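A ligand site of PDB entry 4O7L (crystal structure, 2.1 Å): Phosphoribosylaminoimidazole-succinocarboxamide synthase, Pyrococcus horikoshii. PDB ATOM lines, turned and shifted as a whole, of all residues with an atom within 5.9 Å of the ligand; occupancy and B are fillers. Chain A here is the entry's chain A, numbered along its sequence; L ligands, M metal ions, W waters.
O4 of the ligand sits at hydrogen-bond distance from N of Lys 11, 3.1 Å away.
An oxygen (O5) of the ligand is in salt-bridge range of the side-chain amino group (NZ) of Lys 13, 2.4 Å away.
The backbone NH of Asp 190 lies within hydrogen-bond range of a nitrogen (N2) of the ligand (3.0 Å).
The side-chain carboxylate (OE1) of Glu 177 sits at hydrogen-bond distance from an oxygen (O10) of the ligand.
N3 of the ligand is in hydrogen-bond range of ND1 of His 68, at 2.8 Å.
A nitrogen (N3) of the ligand is in hydrogen-bond range of the backbone carbonyl oxygen (O) of Glu 81 (2.8 Å).
A nitrogen (N4) of the ligand is in hydrogen-bond range of the backbone NH of Leu 83 (3.3 Å).
N of Ala 12 is in hydrogen-bond range of O4 of the ligand (3.0 Å).
O2 of the ligand is in salt-bridge range of NZ of Lys 11 (2.9 Å).
O4 of the ligand is in hydrogen-bond range of N of Lys 13 (3.0 Å).
The side-chain hydroxyl (OH) of Tyr 8 is in hydrogen-bond range of an oxygen (O3) of the ligand, 2.7 Å away.
The side-chain amino group (NZ) of Lys 122 lies within salt-bridge range of an oxygen (O1) of the ligand, at 3.8 Å.
NZ of Lys 13 lies within salt-bridge range of OD2 of Asp 190 (2.7 Å).
O of Tyr 8 sits at hydrogen-bond distance from N of Met 15, at 2.8 Å.
The backbone NH (N) of Ala 189 lies within hydrogen-bond range of the backbone carbonyl oxygen (O) of Glu 177 (2.8 Å).
OE2 of Glu 177 is in salt-bridge range of NZ of Lys 122 (3.2 Å).
NZ of Lys 13 is in salt-bridge range of OE2 of Glu 191, at 3.0 Å.
NE2 of His 68 sits at hydrogen-bond distance from O of Asp 190.
The backbone NH (N) of Glu 81 lies within hydrogen-bond range of the backbone carbonyl oxygen (O) of His 68 (2.8 Å).
The side-chain sulfur (SD) of Met 15 sits close to an oxygen (O8) of the ligand.
The side-chain sulfur of Met 85 lies close to a nitrogen (N5) of the ligand, at 3.7 Å.
Gly 10 touches the ligand.
Ala 189 touches the ligand.
The nearest printed residue that does not touch the ligand is Lys 82 (4.01 Å).
Water W1 lies within hydrogen-bond range of the side-chain carboxylate (OD2) of Asp 190 (2.8 Å), the side-chain carboxylate (OE2) of Glu 177 (2.9 Å) and an oxygen (O5) of the ligand (3.2 Å).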
ATOM      1  N   TYR A   8      19.451  13.899  -6.141  1.00  0.00           N
ATOM      2  CA  TYR A   8      19.103  15.203  -5.569  1.00  0.00           C
ATOM      3  C   TYR A   8      18.385  16.038  -6.645  1.00  0.00           C
ATOM      4  O   TYR A   8      18.911  16.241  -7.743  1.00  0.00           O
ATOM      5  CB  TYR A   8      20.358  15.921  -5.032  1.00  0.00           C
ATOM      6  CG  TYR A   8      20.128  17.365  -4.605  1.00  0.00           C
ATOM      7  CD1 TYR A   8      19.792  17.687  -3.285  1.00  0.00           C
ATOM      8  CD2 TYR A   8      20.234  18.415  -5.537  1.00  0.00           C
ATOM      9  CE1 TYR A   8      19.564  19.000  -2.899  1.00  0.00           C
ATOM     10  CE2 TYR A   8      20.016  19.732  -5.160  1.00  0.00           C
ATOM     11  CZ  TYR A   8      19.685  20.017  -3.840  1.00  0.00           C
ATOM     12  OH  TYR A   8      19.466  21.331  -3.477  1.00  0.00           O
ATOM     13  N   GLU A   9      17.182  16.509  -6.322  1.00  0.00           N
ATOM     14  CA  GLU A   9      16.418  17.369  -7.225  1.00  0.00           C
ATOM     15  C   GLU A   9      16.417  18.813  -6.712  1.00  0.00           C
ATOM     16  O   GLU A   9      15.817  19.114  -5.674  1.00  0.00           O
ATOM     17  CB  GLU A   9      14.989  16.847  -7.416  1.00  0.00           C
ATOM     18  N   GLY A  10      17.102  19.702  -7.441  1.00  0.00           N
ATOM     19  CA  GLY A  10      17.116  21.128  -7.120  1.00  0.00           C
ATOM     20  C   GLY A  10      16.080  21.920  -7.892  1.00  0.00           C
ATOM     21  O   GLY A  10      15.254  21.332  -8.601  1.00  0.00           O
ATOM     22  N   LYS A  11      16.129  23.250  -7.780  1.00  0.00           N
ATOM     23  CA  LYS A  11      15.206  24.123  -8.519  1.00  0.00           C
ATOM     24  C   LYS A  11      15.434  24.106 -10.047  1.00  0.00           C
ATOM     25  O   LYS A  11      14.469  24.163 -10.830  1.00  0.00           O
ATOM     26  CB  LYS A  11      15.256  25.561  -7.973  1.00  0.00           C
ATOM     27  CG  LYS A  11      14.803  25.681  -6.524  1.00  0.00           C
ATOM     28  CD  LYS A  11      14.606  27.122  -6.064  1.00  0.00           C
ATOM     29  CE  LYS A  11      15.873  27.959  -6.157  1.00  0.00           C
ATOM     30  NZ  LYS A  11      17.069  27.273  -5.600  1.00  0.00           N
ATOM     31  N   ALA A  12      16.696  24.008 -10.468  1.00  0.00           N
ATOM     32  CA  ALA A  12      17.023  24.006 -11.899  1.00  0.00           C
ATOM     33  C   ALA A  12      17.604  22.695 -12.447  1.00  0.00           C
ATOM     34  O   ALA A  12      17.532  22.429 -13.640  1.00  0.00           O
ATOM     35  N   LYS A  13      18.202  21.892 -11.568  1.00  0.00           N
ATOM     36  CA  LYS A  13      18.934  20.694 -12.014  1.00  0.00           C
ATOM     37  C   LYS A  13      18.700  19.450 -11.143  1.00  0.00           C
ATOM     38  O   LYS A  13      18.276  19.554  -9.983  1.00  0.00           O
ATOM     39  CB  LYS A  13      20.453  20.984 -12.171  1.00  0.00           C
ATOM     40  CG  LYS A  13      20.795  22.201 -13.047  1.00  0.00           C
ATOM     41  CD  LYS A  13      22.275  22.395 -13.304  1.00  0.00           C
ATOM     42  CE  LYS A  13      23.103  22.602 -12.031  1.00  0.00           C
ATOM     43  NZ  LYS A  13      22.844  23.896 -11.321  1.00  0.00           N
ATOM     44  N   LYS A  14      18.962  18.276 -11.725  1.00  0.00           N
ATOM     45  CA  LYS A  14      18.988  17.007 -10.988  1.00  0.00           C
ATOM     46  C   LYS A  14      20.431  16.459 -10.913  1.00  0.00           C
ATOM     47  O   LYS A  14      21.153  16.478 -11.914  1.00  0.00           O
ATOM     48  N   MET A  15      20.836  15.989  -9.741  1.00  0.00           N
ATOM     49  CA  MET A  15      22.157  15.381  -9.564  1.00  0.00           C
ATOM     50  C   MET A  15      21.997  13.899  -9.262  1.00  0.00           C
ATOM     51  O   MET A  15      21.478  13.528  -8.205  1.00  0.00           O
ATOM     52  CB  MET A  15      22.945  16.085  -8.440  1.00  0.00           C
ATOM     53  CG  MET A  15      23.002  17.609  -8.546  1.00  0.00           C
ATOM     54  SD  MET A  15      23.707  18.201 -10.102  1.00  0.00           S
ATOM     55  CE  MET A  15      25.464  18.177  -9.744  1.00  0.00           C
ATOM     56  N   LEU A  23      28.926  12.016 -10.753  1.00  0.00           N
ATOM     57  CA  LEU A  23      27.476  12.087 -10.823  1.00  0.00           C
ATOM     58  C   LEU A  23      26.996  12.617 -12.173  1.00  0.00           C
ATOM     59  O   LEU A  23      27.790  13.052 -13.014  1.00  0.00           O
ATOM     60  CB  LEU A  23      26.883  12.848  -9.620  1.00  0.00           C
ATOM     61  CG  LEU A  23      27.132  14.332  -9.353  1.00  0.00           C
ATOM     62  CD1 LEU A  23      26.237  14.814  -8.222  1.00  0.00           C
ATOM     63  CD2 LEU A  23      28.574  14.617  -8.996  1.00  0.00           C
ATOM     64  N   MET A  25      24.724  15.408 -13.920  1.00  0.00           N
ATOM     65  CA  MET A  25      24.067  16.706 -13.731  1.00  0.00           C
ATOM     66  C   MET A  25      23.063  16.875 -14.850  1.00  0.00           C
ATOM     67  O   MET A  25      23.429  17.038 -16.013  1.00  0.00           O
ATOM     68  CB  MET A  25      25.094  17.841 -13.736  1.00  0.00           C
ATOM     69  CG  MET A  25      24.490  19.227 -13.511  1.00  0.00           C
ATOM     70  SD  MET A  25      25.750  20.445 -13.047  1.00  0.00           S
ATOM     71  CE  MET A  25      26.722  20.544 -14.533  1.00  0.00           C
ATOM     72  N   HIS A  68      34.625  20.575 -12.841  1.00  0.00           N
ATOM     73  CA  HIS A  68      34.093  19.234 -12.618  1.00  0.00           C
ATOM     74  C   HIS A  68      33.647  18.516 -13.880  1.00  0.00           C
ATOM     75  O   HIS A  68      33.285  17.339 -13.833  1.00  0.00           O
ATOM     76  CB  HIS A  68      32.967  19.281 -11.579  1.00  0.00           C
ATOM     77  CG  HIS A  68      31.707  19.980 -12.067  1.00  0.00           C
ATOM     78  ND1 HIS A  68      30.519  19.828 -11.439  1.00  0.00           N
ATOM     79  CD2 HIS A  68      31.477  20.842 -13.142  1.00  0.00           C
ATOM     80  CE1 HIS A  68      29.574  20.550 -12.076  1.00  0.00           C
ATOM     81  NE2 HIS A  68      30.155  21.171 -13.121  1.00  0.00           N
ATOM     82  N   VAL A  80      29.811  14.665 -14.406  1.00  0.00           N
ATOM     83  CA  VAL A  80      30.677  15.567 -13.666  1.00  0.00           C
ATOM     84  C   VAL A  80      31.319  14.867 -12.464  1.00  0.00           C
ATOM     85  O   VAL A  80      30.747  13.925 -11.901  1.00  0.00           O
ATOM     86  CB  VAL A  80      29.948  16.857 -13.194  1.00  0.00           C
ATOM     87  CG1 VAL A  80      29.548  17.720 -14.391  1.00  0.00           C
ATOM     88  CG2 VAL A  80      28.724  16.530 -12.335  1.00  0.00           C
ATOM     89  N   GLU A  81      32.493  15.344 -12.090  1.00  0.00           N
ATOM     90  CA  GLU A  81      33.155  14.890 -10.879  1.00  0.00           C
ATOM     91  C   GLU A  81      32.400  15.288  -9.621  1.00  0.00           C
ATOM     92  O   GLU A  81      31.996  16.443  -9.464  1.00  0.00           O
ATOM     93  CB  GLU A  81      34.553  15.491 -10.852  1.00  0.00           C
ATOM     94  CG  GLU A  81      35.436  14.929  -9.770  1.00  0.00           C
ATOM     95  CD  GLU A  81      36.784  15.622  -9.742  1.00  0.00           C
ATOM     96  OE1 GLU A  81      36.917  16.713 -10.344  1.00  0.00           O
ATOM     97  OE2 GLU A  81      37.690  15.078  -9.107  1.00  0.00           O
ATOM     98  N   LYS A  82      32.233  14.327  -8.716  1.00  0.00           N
ATOM     99  CA  LYS A  82      31.625  14.586  -7.417  1.00  0.00           C
ATOM    100  C   LYS A  82      32.614  15.320  -6.511  1.00  0.00           C
ATOM    101  O   LYS A  82      33.787  14.967  -6.442  1.00  0.00           O
ATOM    102  CB  LYS A  82      31.157  13.282  -6.758  1.00  0.00           C
ATOM    103  CG  LYS A  82      30.252  13.475  -5.557  1.00  0.00           C
ATOM    104  CD  LYS A  82      30.095  12.169  -4.775  1.00  0.00           C
ATOM    105  CE  LYS A  82      29.311  12.400  -3.498  1.00  0.00           C
ATOM    106  NZ  LYS A  82      29.355  11.200  -2.617  1.00  0.00           N
ATOM    107  N   LEU A  83      32.151  16.378  -5.853  1.00  0.00           N
ATOM    108  CA  LEU A  83      33.022  17.199  -5.047  1.00  0.00           C
ATOM    109  C   LEU A  83      32.407  17.459  -3.711  1.00  0.00           C
ATOM    110  O   LEU A  83      31.191  17.415  -3.542  1.00  0.00           O
ATOM    111  CB  LEU A  83      33.291  18.541  -5.731  1.00  0.00           C
ATOM    112  CG  LEU A  83      33.879  18.589  -7.137  1.00  0.00           C
ATOM    113  CD1 LEU A  83      33.717  19.990  -7.728  1.00  0.00           C
ATOM    114  CD2 LEU A  83      35.331  18.163  -7.137  1.00  0.00           C
ATOM    115  N   ASP A  84      33.281  17.729  -2.758  1.00  0.00           N
ATOM    116  CA  ASP A  84      32.909  18.267  -1.461  1.00  0.00           C
ATOM    117  C   ASP A  84      32.713  19.761  -1.676  1.00  0.00           C
ATOM    118  O   ASP A  84      33.680  20.515  -1.733  1.00  0.00           O
ATOM    119  CB  ASP A  84      34.030  18.043  -0.450  1.00  0.00           C
ATOM    120  CG  ASP A  84      33.946  16.708   0.266  1.00  0.00           C
ATOM    121  OD1 ASP A  84      34.795  16.472   1.144  1.00  0.00           O
ATOM    122  OD2 ASP A  84      33.041  15.905  -0.035  1.00  0.00           O
ATOM    123  N   MET A  85      31.452  20.180  -1.822  1.00  0.00           N
ATOM    124  CA  MET A  85      31.120  21.560  -2.212  1.00  0.00           C
ATOM    125  C   MET A  85      31.368  22.584  -1.121  1.00  0.00           C
ATOM    126  O   MET A  85      31.154  22.327   0.053  1.00  0.00           O
ATOM    127  CB  MET A  85      29.676  21.664  -2.694  1.00  0.00           C
ATOM    128  CG  MET A  85      29.369  20.837  -3.954  1.00  0.00           C
ATOM    129  SD  MET A  85      30.233  21.379  -5.457  1.00  0.00           S
ATOM    130  CE  MET A  85      29.547  23.041  -5.602  1.00  0.00           C
ATOM    131  N   LYS A 122      25.700  30.026   0.936  1.00  0.00           N
ATOM    132  CA  LYS A 122      24.551  29.209   0.501  1.00  0.00           C
ATOM    133  C   LYS A 122      23.829  28.658   1.711  1.00  0.00           C
ATOM    134  O   LYS A 122      24.329  27.753   2.387  1.00  0.00           O
ATOM    135  CB  LYS A 122      24.997  28.066  -0.406  1.00  0.00           C
ATOM    136  CG  LYS A 122      24.959  28.405  -1.890  1.00  0.00           C
ATOM    137  CD  LYS A 122      25.563  27.287  -2.730  1.00  0.00           C
ATOM    138  CE  LYS A 122      24.591  26.143  -2.960  1.00  0.00           C
ATOM    139  NZ  LYS A 122      23.586  26.510  -3.994  1.00  0.00           N
ATOM    140  N   GLU A 177      30.201  28.340  -8.487  1.00  0.00           N
ATOM    141  CA  GLU A 177      30.282  27.513  -7.283  1.00  0.00           C
ATOM    142  C   GLU A 177      31.498  26.613  -7.388  1.00  0.00           C
ATOM    143  O   GLU A 177      31.936  26.271  -8.505  1.00  0.00           O
ATOM    144  CB  GLU A 177      29.008  26.674  -7.131  1.00  0.00           C
ATOM    145  CG  GLU A 177      27.756  27.488  -6.818  1.00  0.00           C
ATOM    146  CD  GLU A 177      26.555  26.631  -6.460  1.00  0.00           C
ATOM    147  OE1 GLU A 177      26.712  25.430  -6.145  1.00  0.00           O
ATOM    148  OE2 GLU A 177      25.448  27.163  -6.468  1.00  0.00           O
ATOM    149  N   ALA A 189      32.549  24.214 -10.229  1.00  0.00           N
ATOM    150  CA  ALA A 189      31.440  23.260 -10.273  1.00  0.00           C
ATOM    151  C   ALA A 189      30.149  23.837 -10.844  1.00  0.00           C
ATOM    152  O   ALA A 189      30.183  24.801 -11.629  1.00  0.00           O
ATOM    153  CB  ALA A 189      31.218  22.662  -8.883  1.00  0.00           C
ATOM    154  N   ASP A 190      29.019  23.229 -10.474  1.00  0.00           N
ATOM    155  CA  ASP A 190      27.695  23.690 -10.883  1.00  0.00           C
ATOM    156  C   ASP A 190      27.616  23.961 -12.401  1.00  0.00           C
ATOM    157  O   ASP A 190      28.119  23.152 -13.204  1.00  0.00           O
ATOM    158  CB  ASP A 190      27.285  24.915 -10.052  1.00  0.00           C
ATOM    159  CG  ASP A 190      25.800  25.205 -10.132  1.00  0.00           C
ATOM    160  OD1 ASP A 190      25.438  26.292 -10.587  1.00  0.00           O
ATOM    161  OD2 ASP A 190      24.993  24.333  -9.741  1.00  0.00           O
ATOM    162  N   GLU A 191      27.029  25.089 -12.808  1.00  0.00           N
ATOM    163  CA  GLU A 191      26.807  25.375 -14.222  1.00  0.00           C
ATOM    164  C   GLU A 191      27.324  26.754 -14.588  1.00  0.00           C
ATOM    165  O   GLU A 191      27.596  27.578 -13.692  1.00  0.00           O
ATOM    166  CB  GLU A 191      25.306  25.265 -14.571  1.00  0.00           C
ATOM    167  CG  GLU A 191      24.464  26.454 -14.084  1.00  0.00           C
ATOM    168  CD  GLU A 191      22.973  26.295 -14.345  1.00  0.00           C
ATOM    169  OE1 GLU A 191      22.513  26.540 -15.477  1.00  0.00           O
ATOM    170  OE2 GLU A 191      22.259  25.954 -13.392  1.00  0.00           O
HETATM  171  P1  LIG L   1      19.562  24.153  -5.964  1.00  0.00           P
HETATM  172  O1  LIG L   1      20.349  24.760  -4.821  1.00  0.00           O
HETATM  173  O2  LIG L   1      18.610  25.097  -6.657  1.00  0.00           O
HETATM  174  O3  LIG L   1      19.003  22.796  -5.656  1.00  0.00           O
HETATM  175  P2  LIG L   1      20.443  23.202  -8.544  1.00  0.00           P
HETATM  176  O4  LIG L   1      18.984  22.989  -8.841  1.00  0.00           O
HETATM  177  O5  LIG L   1      21.222  24.072  -9.502  1.00  0.00           O
HETATM  178  O6  LIG L   1      20.701  23.845  -7.071  1.00  0.00           O
HETATM  179  O7  LIG L   1      21.110  21.732  -8.427  1.00  0.00           O
HETATM  180  C1  LIG L   1      22.528  21.514  -8.420  1.00  0.00           C
HETATM  181  C2  LIG L   1      23.054  21.164  -7.021  1.00  0.00           C
HETATM  182  O8  LIG L   1      24.267  20.387  -7.092  1.00  0.00           O
HETATM  183  C3  LIG L   1      23.430  22.399  -6.220  1.00  0.00           C
HETATM  184  O9  LIG L   1      23.140  22.081  -4.847  1.00  0.00           O
HETATM  185  C4  LIG L   1      24.935  22.537  -6.455  1.00  0.00           C
HETATM  186  O10 LIG L   1      25.608  23.264  -5.425  1.00  0.00           O
HETATM  187  C5  LIG L   1      25.373  21.087  -6.472  1.00  0.00           C
HETATM  188  N1  LIG L   1      26.562  20.783  -7.310  1.00  0.00           N
HETATM  189  C6  LIG L   1      26.939  21.368  -8.466  1.00  0.00           C
HETATM  190  N2  LIG L   1      28.079  20.793  -8.945  1.00  0.00           N
HETATM  191  C7  LIG L   1      28.430  19.808  -8.096  1.00  0.00           C
HETATM  192  C8  LIG L   1      29.514  18.784  -7.986  1.00  0.00           C
HETATM  193  N3  LIG L   1      30.479  18.684  -8.907  1.00  0.00           N
HETATM  194  N4  LIG L   1      29.506  17.957  -6.903  1.00  0.00           N
HETATM  195  C9  LIG L   1      28.557  18.010  -5.953  1.00  0.00           C
HETATM  196  N5  LIG L   1      27.542  18.902  -5.994  1.00  0.00           N
HETATM  197  C10 LIG L   1      27.422  19.806  -7.015  1.00  0.00           C
HETATM  198 MG    MG M   1      21.711  26.322  -8.102  1.00  0.00          MG
HETATM  199  O   HOH W   1      23.477  25.410  -7.677  1.00  0.00           O
HETATM  200  O   HOH W   2      25.932  22.590  -2.848  1.00  0.00           O
